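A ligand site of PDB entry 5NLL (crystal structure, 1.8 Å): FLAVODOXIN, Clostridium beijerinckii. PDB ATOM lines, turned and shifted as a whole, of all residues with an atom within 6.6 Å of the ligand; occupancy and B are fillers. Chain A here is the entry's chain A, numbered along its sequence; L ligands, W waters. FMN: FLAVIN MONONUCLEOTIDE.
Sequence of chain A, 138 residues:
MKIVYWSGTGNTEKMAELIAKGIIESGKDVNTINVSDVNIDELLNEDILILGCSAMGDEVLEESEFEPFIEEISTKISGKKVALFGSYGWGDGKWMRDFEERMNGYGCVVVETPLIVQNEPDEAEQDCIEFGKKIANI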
ATOM      1  N   TRP A   6      17.172 -35.209  31.669  1.00  0.00           N
ATOM      2  CA  TRP A   6      18.300 -36.121  31.551  1.00  0.00           C
ATOM      3  C   TRP A   6      19.476 -35.313  32.086  1.00  0.00           C
ATOM      4  O   TRP A   6      19.575 -34.107  31.792  1.00  0.00           O
ATOM      5  CB  TRP A   6      18.605 -36.534  30.109  1.00  0.00           C
ATOM      6  CG  TRP A   6      19.763 -37.523  30.049  1.00  0.00           C
ATOM      7  CD1 TRP A   6      19.681 -38.890  30.163  1.00  0.00           C
ATOM      8  CD2 TRP A   6      21.163 -37.219  29.954  1.00  0.00           C
ATOM      9  NE1 TRP A   6      20.941 -39.446  30.169  1.00  0.00           N
ATOM     10  CE2 TRP A   6      21.872 -38.447  30.031  1.00  0.00           C
ATOM     11  CE3 TRP A   6      21.901 -36.021  29.809  1.00  0.00           C
ATOM     12  CZ2 TRP A   6      23.280 -38.511  29.983  1.00  0.00           C
ATOM     13  CZ3 TRP A   6      23.306 -36.085  29.747  1.00  0.00           C
ATOM     14  CH2 TRP A   6      23.968 -37.326  29.839  1.00  0.00           C
ATOM     15  N   SER A   7      20.315 -35.936  32.895  1.00  0.00           N
ATOM     16  CA  SER A   7      21.473 -35.242  33.429  1.00  0.00           C
ATOM     17  C   SER A   7      22.624 -36.222  33.571  1.00  0.00           C
ATOM     18  O   SER A   7      22.434 -37.298  34.133  1.00  0.00           O
ATOM     19  CB  SER A   7      21.098 -34.619  34.773  1.00  0.00           C
ATOM     20  OG  SER A   7      22.216 -33.952  35.335  1.00  0.00           O
ATOM     21  N   GLY A   8      23.795 -35.863  33.041  1.00  0.00           N
ATOM     22  CA  GLY A   8      24.963 -36.730  33.104  1.00  0.00           C
ATOM     23  C   GLY A   8      25.875 -36.564  34.323  1.00  0.00           C
ATOM     24  O   GLY A   8      26.591 -37.495  34.693  1.00  0.00           O
ATOM     25  N   THR A   9      25.892 -35.371  34.910  1.00  0.00           N
ATOM     26  CA  THR A   9      26.722 -35.151  36.093  1.00  0.00           C
ATOM     27  C   THR A   9      25.902 -34.553  37.250  1.00  0.00           C
ATOM     28  O   THR A   9      26.422 -34.352  38.361  1.00  0.00           O
ATOM     29  CB  THR A   9      27.962 -34.243  35.803  1.00  0.00           C
ATOM     30  OG1 THR A   9      27.552 -32.882  35.674  1.00  0.00           O
ATOM     31  CG2 THR A   9      28.661 -34.679  34.512  1.00  0.00           C
ATOM     32  N   GLY A  10      24.635 -34.252  36.995  1.00  0.00           N
ATOM     33  CA  GLY A  10      23.787 -33.708  38.033  1.00  0.00           C
ATOM     34  C   GLY A  10      23.453 -32.240  37.909  1.00  0.00           C
ATOM     35  O   GLY A  10      22.687 -31.741  38.711  1.00  0.00           O
ATOM     36  N   ASN A  11      23.977 -31.548  36.905  1.00  0.00           N
ATOM     37  CA  ASN A  11      23.701 -30.118  36.771  1.00  0.00           C
ATOM     38  C   ASN A  11      22.256 -29.831  36.386  1.00  0.00           C
ATOM     39  O   ASN A  11      21.582 -29.046  37.059  1.00  0.00           O
ATOM     40  CB  ASN A  11      24.694 -29.456  35.819  1.00  0.00           C
ATOM     41  CG  ASN A  11      26.105 -29.473  36.366  1.00  0.00           C
ATOM     42  OD1 ASN A  11      26.304 -29.594  37.577  1.00  0.00           O
ATOM     43  ND2 ASN A  11      27.085 -29.388  35.473  1.00  0.00           N
ATOM     44  N   THR A  12      21.741 -30.512  35.363  1.00  0.00           N
ATOM     45  CA  THR A  12      20.357 -30.335  34.937  1.00  0.00           C
ATOM     46  C   THR A  12      19.390 -30.895  35.980  1.00  0.00           C
ATOM     47  O   THR A  12      18.280 -30.401  36.149  1.00  0.00           O
ATOM     48  CB  THR A  12      20.093 -30.983  33.566  1.00  0.00           C
ATOM     49  OG1 THR A  12      20.981 -30.387  32.608  1.00  0.00           O
ATOM     50  CG2 THR A  12      18.642 -30.755  33.124  1.00  0.00           C
ATOM     51  N   GLU A  13      19.818 -31.939  36.666  1.00  0.00           N
ATOM     52  CA  GLU A  13      19.028 -32.551  37.722  1.00  0.00           C
ATOM     53  C   GLU A  13      18.795 -31.520  38.818  1.00  0.00           C
ATOM     54  O   GLU A  13      17.685 -31.377  39.322  1.00  0.00           O
ATOM     55  CB  GLU A  13      19.757 -33.755  38.298  1.00  0.00           C
ATOM     56  CG  GLU A  13      18.972 -34.415  39.396  1.00  0.00           C
ATOM     57  CD  GLU A  13      19.512 -35.780  39.726  1.00  0.00           C
ATOM     58  OE1 GLU A  13      20.637 -35.879  40.245  1.00  0.00           O
ATOM     59  OE2 GLU A  13      18.798 -36.763  39.457  1.00  0.00           O
ATOM     60  N   CYS A  53      17.496 -30.948  29.463  1.00  0.00           N
ATOM     61  CA  CYS A  53      18.599 -31.805  29.042  1.00  0.00           C
ATOM     62  C   CYS A  53      19.800 -30.923  28.779  1.00  0.00           C
ATOM     63  O   CYS A  53      19.659 -29.848  28.191  1.00  0.00           O
ATOM     64  CB  CYS A  53      18.254 -32.546  27.746  1.00  0.00           C
ATOM     65  SG  CYS A  53      19.523 -33.732  27.226  1.00  0.00           S
ATOM     66  N   SER A  54      20.962 -31.368  29.240  1.00  0.00           N
ATOM     67  CA  SER A  54      22.203 -30.637  29.046  1.00  0.00           C
ATOM     68  C   SER A  54      22.678 -30.697  27.593  1.00  0.00           C
ATOM     69  O   SER A  54      22.217 -31.531  26.800  1.00  0.00           O
ATOM     70  CB  SER A  54      23.293 -31.197  29.946  1.00  0.00           C
ATOM     71  OG  SER A  54      23.289 -32.607  29.874  1.00  0.00           O
ATOM     72  N   ALA A  55      23.630 -29.818  27.269  1.00  0.00           N
ATOM     73  CA  ALA A  55      24.189 -29.748  25.935  1.00  0.00           C
ATOM     74  C   ALA A  55      25.197 -30.883  25.716  1.00  0.00           C
ATOM     75  O   ALA A  55      26.193 -30.968  26.435  1.00  0.00           O
ATOM     76  CB  ALA A  55      24.861 -28.395  25.711  1.00  0.00           C
ATOM     77  N   MET A  56      24.904 -31.781  24.773  1.00  0.00           N
ATOM     78  CA  MET A  56      25.835 -32.852  24.431  1.00  0.00           C
ATOM     79  C   MET A  56      26.545 -32.538  23.108  1.00  0.00           C
ATOM     80  O   MET A  56      26.215 -31.563  22.448  1.00  0.00           O
ATOM     81  CB  MET A  56      25.143 -34.215  24.421  1.00  0.00           C
ATOM     82  CG  MET A  56      24.782 -34.709  25.821  1.00  0.00           C
ATOM     83  SD  MET A  56      26.223 -34.915  26.917  1.00  0.00           S
ATOM     84  CE  MET A  56      25.857 -33.650  28.132  1.00  0.00           C
ATOM     85  N   GLY A  57      27.540 -33.328  22.742  1.00  0.00           N
ATOM     86  CA  GLY A  57      28.307 -33.026  21.545  1.00  0.00           C
ATOM     87  C   GLY A  57      27.694 -33.398  20.215  1.00  0.00           C
ATOM     88  O   GLY A  57      27.251 -34.531  20.021  1.00  0.00           O
ATOM     89  N   ASP A  58      27.625 -32.463  19.283  1.00  0.00           N
ATOM     90  CA  ASP A  58      28.116 -31.121  19.497  1.00  0.00           C
ATOM     91  C   ASP A  58      26.924 -30.185  19.396  1.00  0.00           C
ATOM     92  O   ASP A  58      26.387 -29.967  18.313  1.00  0.00           O
ATOM     93  CB  ASP A  58      29.115 -30.783  18.421  1.00  0.00           C
ATOM     94  CG  ASP A  58      29.996 -29.654  18.824  1.00  0.00           C
ATOM     95  OD1 ASP A  58      30.984 -29.962  19.532  1.00  0.00           O
ATOM     96  OD2 ASP A  58      29.688 -28.485  18.481  1.00  0.00           O
ATOM     97  N   GLU A  59      26.531 -29.619  20.534  1.00  0.00           N
ATOM     98  CA  GLU A  59      25.380 -28.744  20.612  1.00  0.00           C
ATOM     99  C   GLU A  59      24.111 -29.499  20.187  1.00  0.00           C
ATOM    100  O   GLU A  59      23.329 -28.985  19.387  1.00  0.00           O
ATOM    101  CB  GLU A  59      25.544 -27.470  19.773  1.00  0.00           C
ATOM    102  CG  GLU A  59      26.651 -26.516  20.250  1.00  0.00           C
ATOM    103  CD  GLU A  59      26.454 -26.028  21.677  1.00  0.00           C
ATOM    104  OE1 GLU A  59      25.304 -25.930  22.157  1.00  0.00           O
ATOM    105  OE2 GLU A  59      27.459 -25.713  22.326  1.00  0.00           O
ATOM    106  N   VAL A  60      23.935 -30.697  20.722  1.00  0.00           N
ATOM    107  CA  VAL A  60      22.755 -31.513  20.432  1.00  0.00           C
ATOM    108  C   VAL A  60      22.191 -32.073  21.754  1.00  0.00           C
ATOM    109  O   VAL A  60      22.830 -31.971  22.801  1.00  0.00           O
ATOM    110  CB  VAL A  60      23.048 -32.717  19.480  1.00  0.00           C
ATOM    111  CG1 VAL A  60      23.557 -32.239  18.150  1.00  0.00           C
ATOM    112  CG2 VAL A  60      24.008 -33.695  20.111  1.00  0.00           C
ATOM    113  N   GLY A  86      18.059 -26.448  30.684  1.00  0.00           N
ATOM    114  CA  GLY A  86      19.202 -27.339  30.657  1.00  0.00           C
ATOM    115  C   GLY A  86      20.492 -26.637  30.998  1.00  0.00           C
ATOM    116  O   GLY A  86      20.551 -25.407  30.941  1.00  0.00           O
ATOM    117  N   SER A  87      21.495 -27.414  31.376  1.00  0.00           N
ATOM    118  CA  SER A  87      22.803 -26.858  31.725  1.00  0.00           C
ATOM    119  C   SER A  87      23.714 -27.063  30.521  1.00  0.00           C
ATOM    120  O   SER A  87      23.514 -27.992  29.741  1.00  0.00           O
ATOM    121  CB  SER A  87      23.384 -27.582  32.939  1.00  0.00           C
ATOM    122  OG  SER A  87      24.662 -27.084  33.291  1.00  0.00           O
ATOM    123  N   TYR A  88      24.708 -26.174  30.356  1.00  0.00           N
ATOM    124  CA  TYR A  88      25.672 -26.278  29.275  1.00  0.00           C
ATOM    125  C   TYR A  88      27.050 -25.907  29.794  1.00  0.00           C
ATOM    126  O   TYR A  88      27.165 -25.412  30.920  1.00  0.00           O
ATOM    127  CB  TYR A  88      25.306 -25.378  28.088  1.00  0.00           C
ATOM    128  CG  TYR A  88      25.332 -23.911  28.394  1.00  0.00           C
ATOM    129  CD1 TYR A  88      24.310 -23.312  29.153  1.00  0.00           C
ATOM    130  CD2 TYR A  88      26.353 -23.097  27.914  1.00  0.00           C
ATOM    131  CE1 TYR A  88      24.324 -21.937  29.415  1.00  0.00           C
ATOM    132  CE2 TYR A  88      26.375 -21.712  28.182  1.00  0.00           C
ATOM    133  CZ  TYR A  88      25.357 -21.149  28.933  1.00  0.00           C
ATOM    134  OH  TYR A  88      25.388 -19.802  29.235  1.00  0.00           O
ATOM    135  N   GLY A  89      28.080 -26.195  29.012  1.00  0.00           N
ATOM    136  CA  GLY A  89      29.428 -25.920  29.434  1.00  0.00           C
ATOM    137  C   GLY A  89      30.083 -24.751  28.728  1.00  0.00           C
ATOM    138  O   GLY A  89      29.965 -23.611  29.135  1.00  0.00           O
ATOM    139  N   TRP A  90      30.679 -25.020  27.580  1.00  0.00           N
ATOM    140  CA  TRP A  90      31.426 -24.003  26.849  1.00  0.00           C
ATOM    141  C   TRP A  90      30.741 -23.266  25.709  1.00  0.00           C
ATOM    142  O   TRP A  90      31.299 -22.304  25.172  1.00  0.00           O
ATOM    143  CB  TRP A  90      32.732 -24.617  26.344  1.00  0.00           C
ATOM    144  CG  TRP A  90      32.484 -25.843  25.515  1.00  0.00           C
ATOM    145  CD1 TRP A  90      32.166 -25.874  24.182  1.00  0.00           C
ATOM    146  CD2 TRP A  90      32.503 -27.205  25.950  1.00  0.00           C
ATOM    147  NE1 TRP A  90      31.988 -27.171  23.769  1.00  0.00           N
ATOM    148  CE2 TRP A  90      32.190 -28.011  24.833  1.00  0.00           C
ATOM    149  CE3 TRP A  90      32.760 -27.825  27.182  1.00  0.00           C
ATOM    150  CZ2 TRP A  90      32.124 -29.399  24.916  1.00  0.00           C
ATOM    151  CZ3 TRP A  90      32.682 -29.217  27.252  1.00  0.00           C
ATOM    152  CH2 TRP A  90      32.373 -29.982  26.129  1.00  0.00           C
ATOM    153  N   GLY A  91      29.550 -23.701  25.309  1.00  0.00           N
ATOM    154  CA  GLY A  91      28.880 -23.074  24.186  1.00  0.00           C
ATOM    155  C   GLY A  91      28.111 -21.827  24.556  1.00  0.00           C
ATOM    156  O   GLY A  91      28.293 -21.270  25.644  1.00  0.00           O
ATOM    157  N   ASP A  92      27.233 -21.380  23.662  1.00  0.00           N
ATOM    158  CA  ASP A  92      26.410 -20.198  23.932  1.00  0.00           C
ATOM    159  C   ASP A  92      24.926 -20.474  23.840  1.00  0.00           C
ATOM    160  O   ASP A  92      24.128 -19.577  23.561  1.00  0.00           O
ATOM    161  CB  ASP A  92      26.796 -19.035  23.019  1.00  0.00           C
ATOM    162  CG  ASP A  92      26.549 -19.315  21.539  1.00  0.00           C
ATOM    163  OD1 ASP A  92      25.986 -20.357  21.166  1.00  0.00           O
ATOM    164  OD2 ASP A  92      26.926 -18.434  20.742  1.00  0.00           O
ATOM    165  N   GLY A  93      24.561 -21.739  24.024  1.00  0.00           N
ATOM    166  CA  GLY A  93      23.165 -22.123  24.001  1.00  0.00           C
ATOM    167  C   GLY A  93      22.615 -22.616  22.680  1.00  0.00           C
ATOM    168  O   GLY A  93      21.398 -22.734  22.550  1.00  0.00           O
ATOM    169  N   TRP A  95      22.423 -25.573  21.360  1.00  0.00           N
ATOM    170  CA  TRP A  95      21.583 -26.758  21.515  1.00  0.00           C
ATOM    171  C   TRP A  95      20.167 -26.368  21.974  1.00  0.00           C
ATOM    172  O   TRP A  95      19.181 -26.987  21.557  1.00  0.00           O
ATOM    173  CB  TRP A  95      22.245 -27.764  22.479  1.00  0.00           C
ATOM    174  CG  TRP A  95      21.672 -27.854  23.880  1.00  0.00           C
ATOM    175  CD1 TRP A  95      20.938 -28.900  24.400  1.00  0.00           C
ATOM    176  CD2 TRP A  95      21.804 -26.895  24.950  1.00  0.00           C
ATOM    177  NE1 TRP A  95      20.624 -28.647  25.711  1.00  0.00           N
ATOM    178  CE2 TRP A  95      21.136 -27.433  26.075  1.00  0.00           C
ATOM    179  CE3 TRP A  95      22.415 -25.642  25.063  1.00  0.00           C
ATOM    180  CZ2 TRP A  95      21.073 -26.759  27.306  1.00  0.00           C
ATOM    181  CZ3 TRP A  95      22.339 -24.964  26.289  1.00  0.00           C
ATOM    182  CH2 TRP A  95      21.675 -25.522  27.391  1.00  0.00           C
ATOM    183  N   VAL A 117      21.631 -22.550  32.073  1.00  0.00           N
ATOM    184  CA  VAL A 117      22.604 -22.181  33.095  1.00  0.00           C
ATOM    185  C   VAL A 117      23.898 -22.903  32.797  1.00  0.00           C
ATOM    186  O   VAL A 117      23.889 -24.073  32.403  1.00  0.00           O
ATOM    187  CB  VAL A 117      22.082 -22.609  34.485  1.00  0.00           C
ATOM    188  CG1 VAL A 117      23.180 -22.500  35.551  1.00  0.00           C
ATOM    189  CG2 VAL A 117      20.852 -21.776  34.861  1.00  0.00           C
ATOM    190  N   GLN A 118      25.016 -22.199  32.944  1.00  0.00           N
ATOM    191  CA  GLN A 118      26.332 -22.771  32.697  1.00  0.00           C
ATOM    192  C   GLN A 118      26.742 -23.586  33.900  1.00  0.00           C
ATOM    193  O   GLN A 118      26.750 -23.072  35.015  1.00  0.00           O
ATOM    194  CB  GLN A 118      27.350 -21.663  32.419  1.00  0.00           C
ATOM    195  CG  GLN A 118      28.756 -22.167  32.159  1.00  0.00           C
ATOM    196  CD  GLN A 118      29.646 -21.142  31.462  1.00  0.00           C
ATOM    197  OE1 GLN A 118      29.376 -19.947  31.515  1.00  0.00           O
ATOM    198  NE2 GLN A 118      30.692 -21.609  30.796  1.00  0.00           N
ATOM    199  N   ASN A 119      27.038 -24.871  33.691  1.00  0.00           N
ATOM    200  CA  ASN A 119      27.445 -25.776  34.770  1.00  0.00           C
ATOM    201  C   ASN A 119      26.449 -25.884  35.930  1.00  0.00           C
ATOM    202  O   ASN A 119      25.244 -25.775  35.703  1.00  0.00           O
ATOM    203  CB  ASN A 119      28.860 -25.439  35.232  1.00  0.00           C
ATOM    204  CG  ASN A 119      29.833 -25.386  34.060  1.00  0.00           C
ATOM    205  OD1 ASN A 119      29.963 -26.342  33.292  1.00  0.00           O
ATOM    206  ND2 ASN A 119      30.455 -24.239  33.883  1.00  0.00           N
ATOM    207  N   GLU A 120      26.915 -26.119  37.146  1.00  0.00           N
ATOM    208  CA  GLU A 120      25.976 -26.270  38.274  1.00  0.00           C
ATOM    209  C   GLU A 120      25.283 -24.957  38.605  1.00  0.00           C
ATOM    210  O   GLU A 120      25.916 -23.912  38.580  1.00  0.00           O
ATOM    211  CB  GLU A 120      26.700 -26.801  39.512  1.00  0.00           C
ATOM    212  CG  GLU A 120      25.774 -27.609  40.428  1.00  0.00           C
ATOM    213  CD  GLU A 120      26.372 -27.926  41.793  1.00  0.00           C
ATOM    214  OE1 GLU A 120      27.499 -28.464  41.835  1.00  0.00           O
ATOM    215  OE2 GLU A 120      25.698 -27.647  42.810  1.00  0.00           O
HETATM  216  N1  FMN L   1      28.597 -28.012  26.612  1.00  0.00           N
HETATM  217  C2  FMN L   1      28.329 -27.108  25.654  1.00  0.00           C
HETATM  218  O2  FMN L   1      28.133 -25.934  25.923  1.00  0.00           O
HETATM  219  N3  FMN L   1      28.234 -27.522  24.305  1.00  0.00           N
HETATM  220  C4  FMN L   1      28.491 -28.783  23.830  1.00  0.00           C
HETATM  221  O4  FMN L   1      28.474 -29.030  22.594  1.00  0.00           O
HETATM  222  C4A FMN L   1      28.809 -29.745  24.887  1.00  0.00           C
HETATM  223  N5  FMN L   1      29.125 -30.965  24.561  1.00  0.00           N
HETATM  224  C5A FMN L   1      29.415 -31.849  25.574  1.00  0.00           C
HETATM  225  C6  FMN L   1      29.743 -33.155  25.230  1.00  0.00           C
HETATM  226  C7  FMN L   1      30.032 -34.088  26.177  1.00  0.00           C
HETATM  227  C7M FMN L   1      30.526 -35.439  25.719  1.00  0.00           C
HETATM  228  C8  FMN L   1      29.919 -33.791  27.557  1.00  0.00           C
HETATM  229  C8M FMN L   1      30.139 -34.855  28.626  1.00  0.00           C
HETATM  230  C9  FMN L   1      29.632 -32.495  27.929  1.00  0.00           C
HETATM  231  C9A FMN L   1      29.341 -31.514  26.955  1.00  0.00           C
HETATM  232  N10 FMN L   1      29.065 -30.191  27.255  1.00  0.00           N
HETATM  233  C10 FMN L   1      28.804 -29.260  26.275  1.00  0.00           C
HETATM  234  C1' FMN L   1      29.123 -29.774  28.661  1.00  0.00           C
HETATM  235  C2' FMN L   1      27.832 -30.079  29.412  1.00  0.00           C
HETATM  236  O2' FMN L   1      26.732 -29.502  28.707  1.00  0.00           O
HETATM  237  C3' FMN L   1      27.918 -29.449  30.789  1.00  0.00           C
HETATM  238  O3' FMN L   1      29.036 -29.995  31.484  1.00  0.00           O
HETATM  239  C4' FMN L   1      26.657 -29.523  31.656  1.00  0.00           C
HETATM  240  O4' FMN L   1      26.871 -28.788  32.865  1.00  0.00           O
HETATM  241  C5' FMN L   1      26.265 -30.976  31.939  1.00  0.00           C
HETATM  242  O5' FMN L   1      25.054 -31.020  32.712  1.00  0.00           O
HETATM  243  P   FMN L   1      24.525 -32.397  33.235  1.00  0.00           P
HETATM  244  O1P FMN L   1      24.788 -33.412  32.171  1.00  0.00           O
HETATM  245  O2P FMN L   1      23.141 -32.128  33.578  1.00  0.00           O
HETATM  246  O3P FMN L   1      25.285 -32.801  34.492  1.00  0.00           O
HETATM  247  O   HOH W   1      25.612 -24.327  24.506  1.00  0.00           O
HETATM  248  O   HOH W   2      27.048 -34.539  31.429  1.00  0.00           O
HETATM  249  O   HOH W   3      31.355 -27.955  21.157  1.00  0.00           O
HETATM  250  O   HOH W   4      28.296 -36.280  23.312  1.00  0.00           O
HETATM  251  O   HOH W   5      29.090 -32.739  31.449  1.00  0.00           O
HETATM  252  O   HOH W   6      29.857 -28.848  33.803  1.00  0.00           O
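Water W6 lies within hydrogen-bond range of OD1 of Asn 119, O3' of the ligand and ND2 of Asn 11. Water W1 lies within hydrogen-bond range of N of Gly 93, OE1 of Glu 59, O2 of the ligand and N of Asp 92. Water W3 lies within hydrogen-bond range of the side-chain carboxylate of Asp 58 (2.6 Å), the indole nitrogen of Trp 90 (2.8 Å) and an oxygen (O4) of the ligand (3.4 Å).
OG1 of Thr 12 lies within hydrogen-bond range of O2P of the ligand (2.9 Å). N of Asn 11 sits at hydrogen-bond distance from O3P of the ligand, at 3.0 Å. N of Gly 57 lies close to N5 of the ligand (3.4 Å). The side-chain carboxylate (OE2) of Glu 59 is in hydrogen-bond range of a nitrogen (N3) of the ligand (2.8 Å). The backbone NH (N) of Gly 10 sits at hydrogen-bond distance from an oxygen (O3P) of the ligand (3.0 Å). O of Ala 55 sits at hydrogen-bond distance from O2' of the ligand, at 2.8 Å. The side-chain hydroxyl (OG1) of Thr 9 sits at hydrogen-bond distance from an oxygen (O3P) of the ligand (2.6 Å). The backbone NH (N) of Thr 9 sits at hydrogen-bond distance from an oxygen (O3P) of the ligand, at 2.7 Å. The side-chain hydroxyl of Ser 7 lies within hydrogen-bond range of an oxygen (O2P) of the ligand (2.7 Å). The side-chain hydroxyl of Ser 54 is in hydrogen-bond range of an oxygen (O1P) of the ligand (2.9 Å). The backbone NH (N) of Glu 59 sits at hydrogen-bond distance from an oxygen (O4) of the ligand. N of Trp 90 is in hydrogen-bond range of O2 of the ligand (3.2 Å). N of Ala 55 lies within hydrogen-bond range of O2' of the ligand. An oxygen (O2) of the ligand sits at hydrogen-bond distance from the backbone NH (N) of Gly 91 (2.7 Å). O4' of the ligand is in hydrogen-bond range of ND2 of Asn 11 (2.7 Å). An oxygen (O4') of the ligand lies within hydrogen-bond range of the side-chain hydroxyl (OG) of Ser 87. The backbone NH of Gly 89 is in hydrogen-bond range of a nitrogen (N1) of the ligand. The backbone NH of Thr 12 sits at hydrogen-bond distance from an oxygen (O2P) of the ligand (2.8 Å). N of Gly 8 is in hydrogen-bond range of O1P of the ligand (2.8 Å).
The backbone carbonyl oxygen (O) of Met 56 lies close to an oxygen (O4) of the ligand (3.4 Å). Trp 6 touches the ligand (CZ3 to O1P, 3.9 Å). Asp 58 touches the ligand (C to O4, 3.7 Å). CA of Tyr 88 touches O2' of the ligand, 3.4 Å away. Asn 119 touches the ligand (CA to O4', 3.6 Å). Hydrophobic or aromatic side chains that line the ligand: Trp 6, Ala 55, Met 56, Tyr 88 and Trp 90.
O of Gly 89 is in hydrogen-bond range of NE2 of Gln 118, at 2.7 Å. The backbone NH (N) of Trp 95 is in hydrogen-bond range of the side-chain carboxylate (OE1) of Glu 59 (3.0 Å). The side-chain hydroxyl (OG) of Ser 7 lies within hydrogen-bond range of the backbone NH (N) of Gly 10, 2.9 Å away. N of Thr 12 is in hydrogen-bond range of OG of Ser 7 (3.5 Å). OG of Ser 7 sits at hydrogen-bond distance from N of Glu 13, at 3.4 Å. The backbone carbonyl oxygen (O) of Val 117 is in hydrogen-bond range of the backbone NH (N) of Tyr 88 (3.0 Å). The backbone carbonyl oxygen (O) of Ser 54 sits close to the indole nitrogen (NE1) of Trp 95 (3.5 Å). OG of Ser 87 lies within hydrogen-bond range of O of Asn 119 (2.8 Å).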
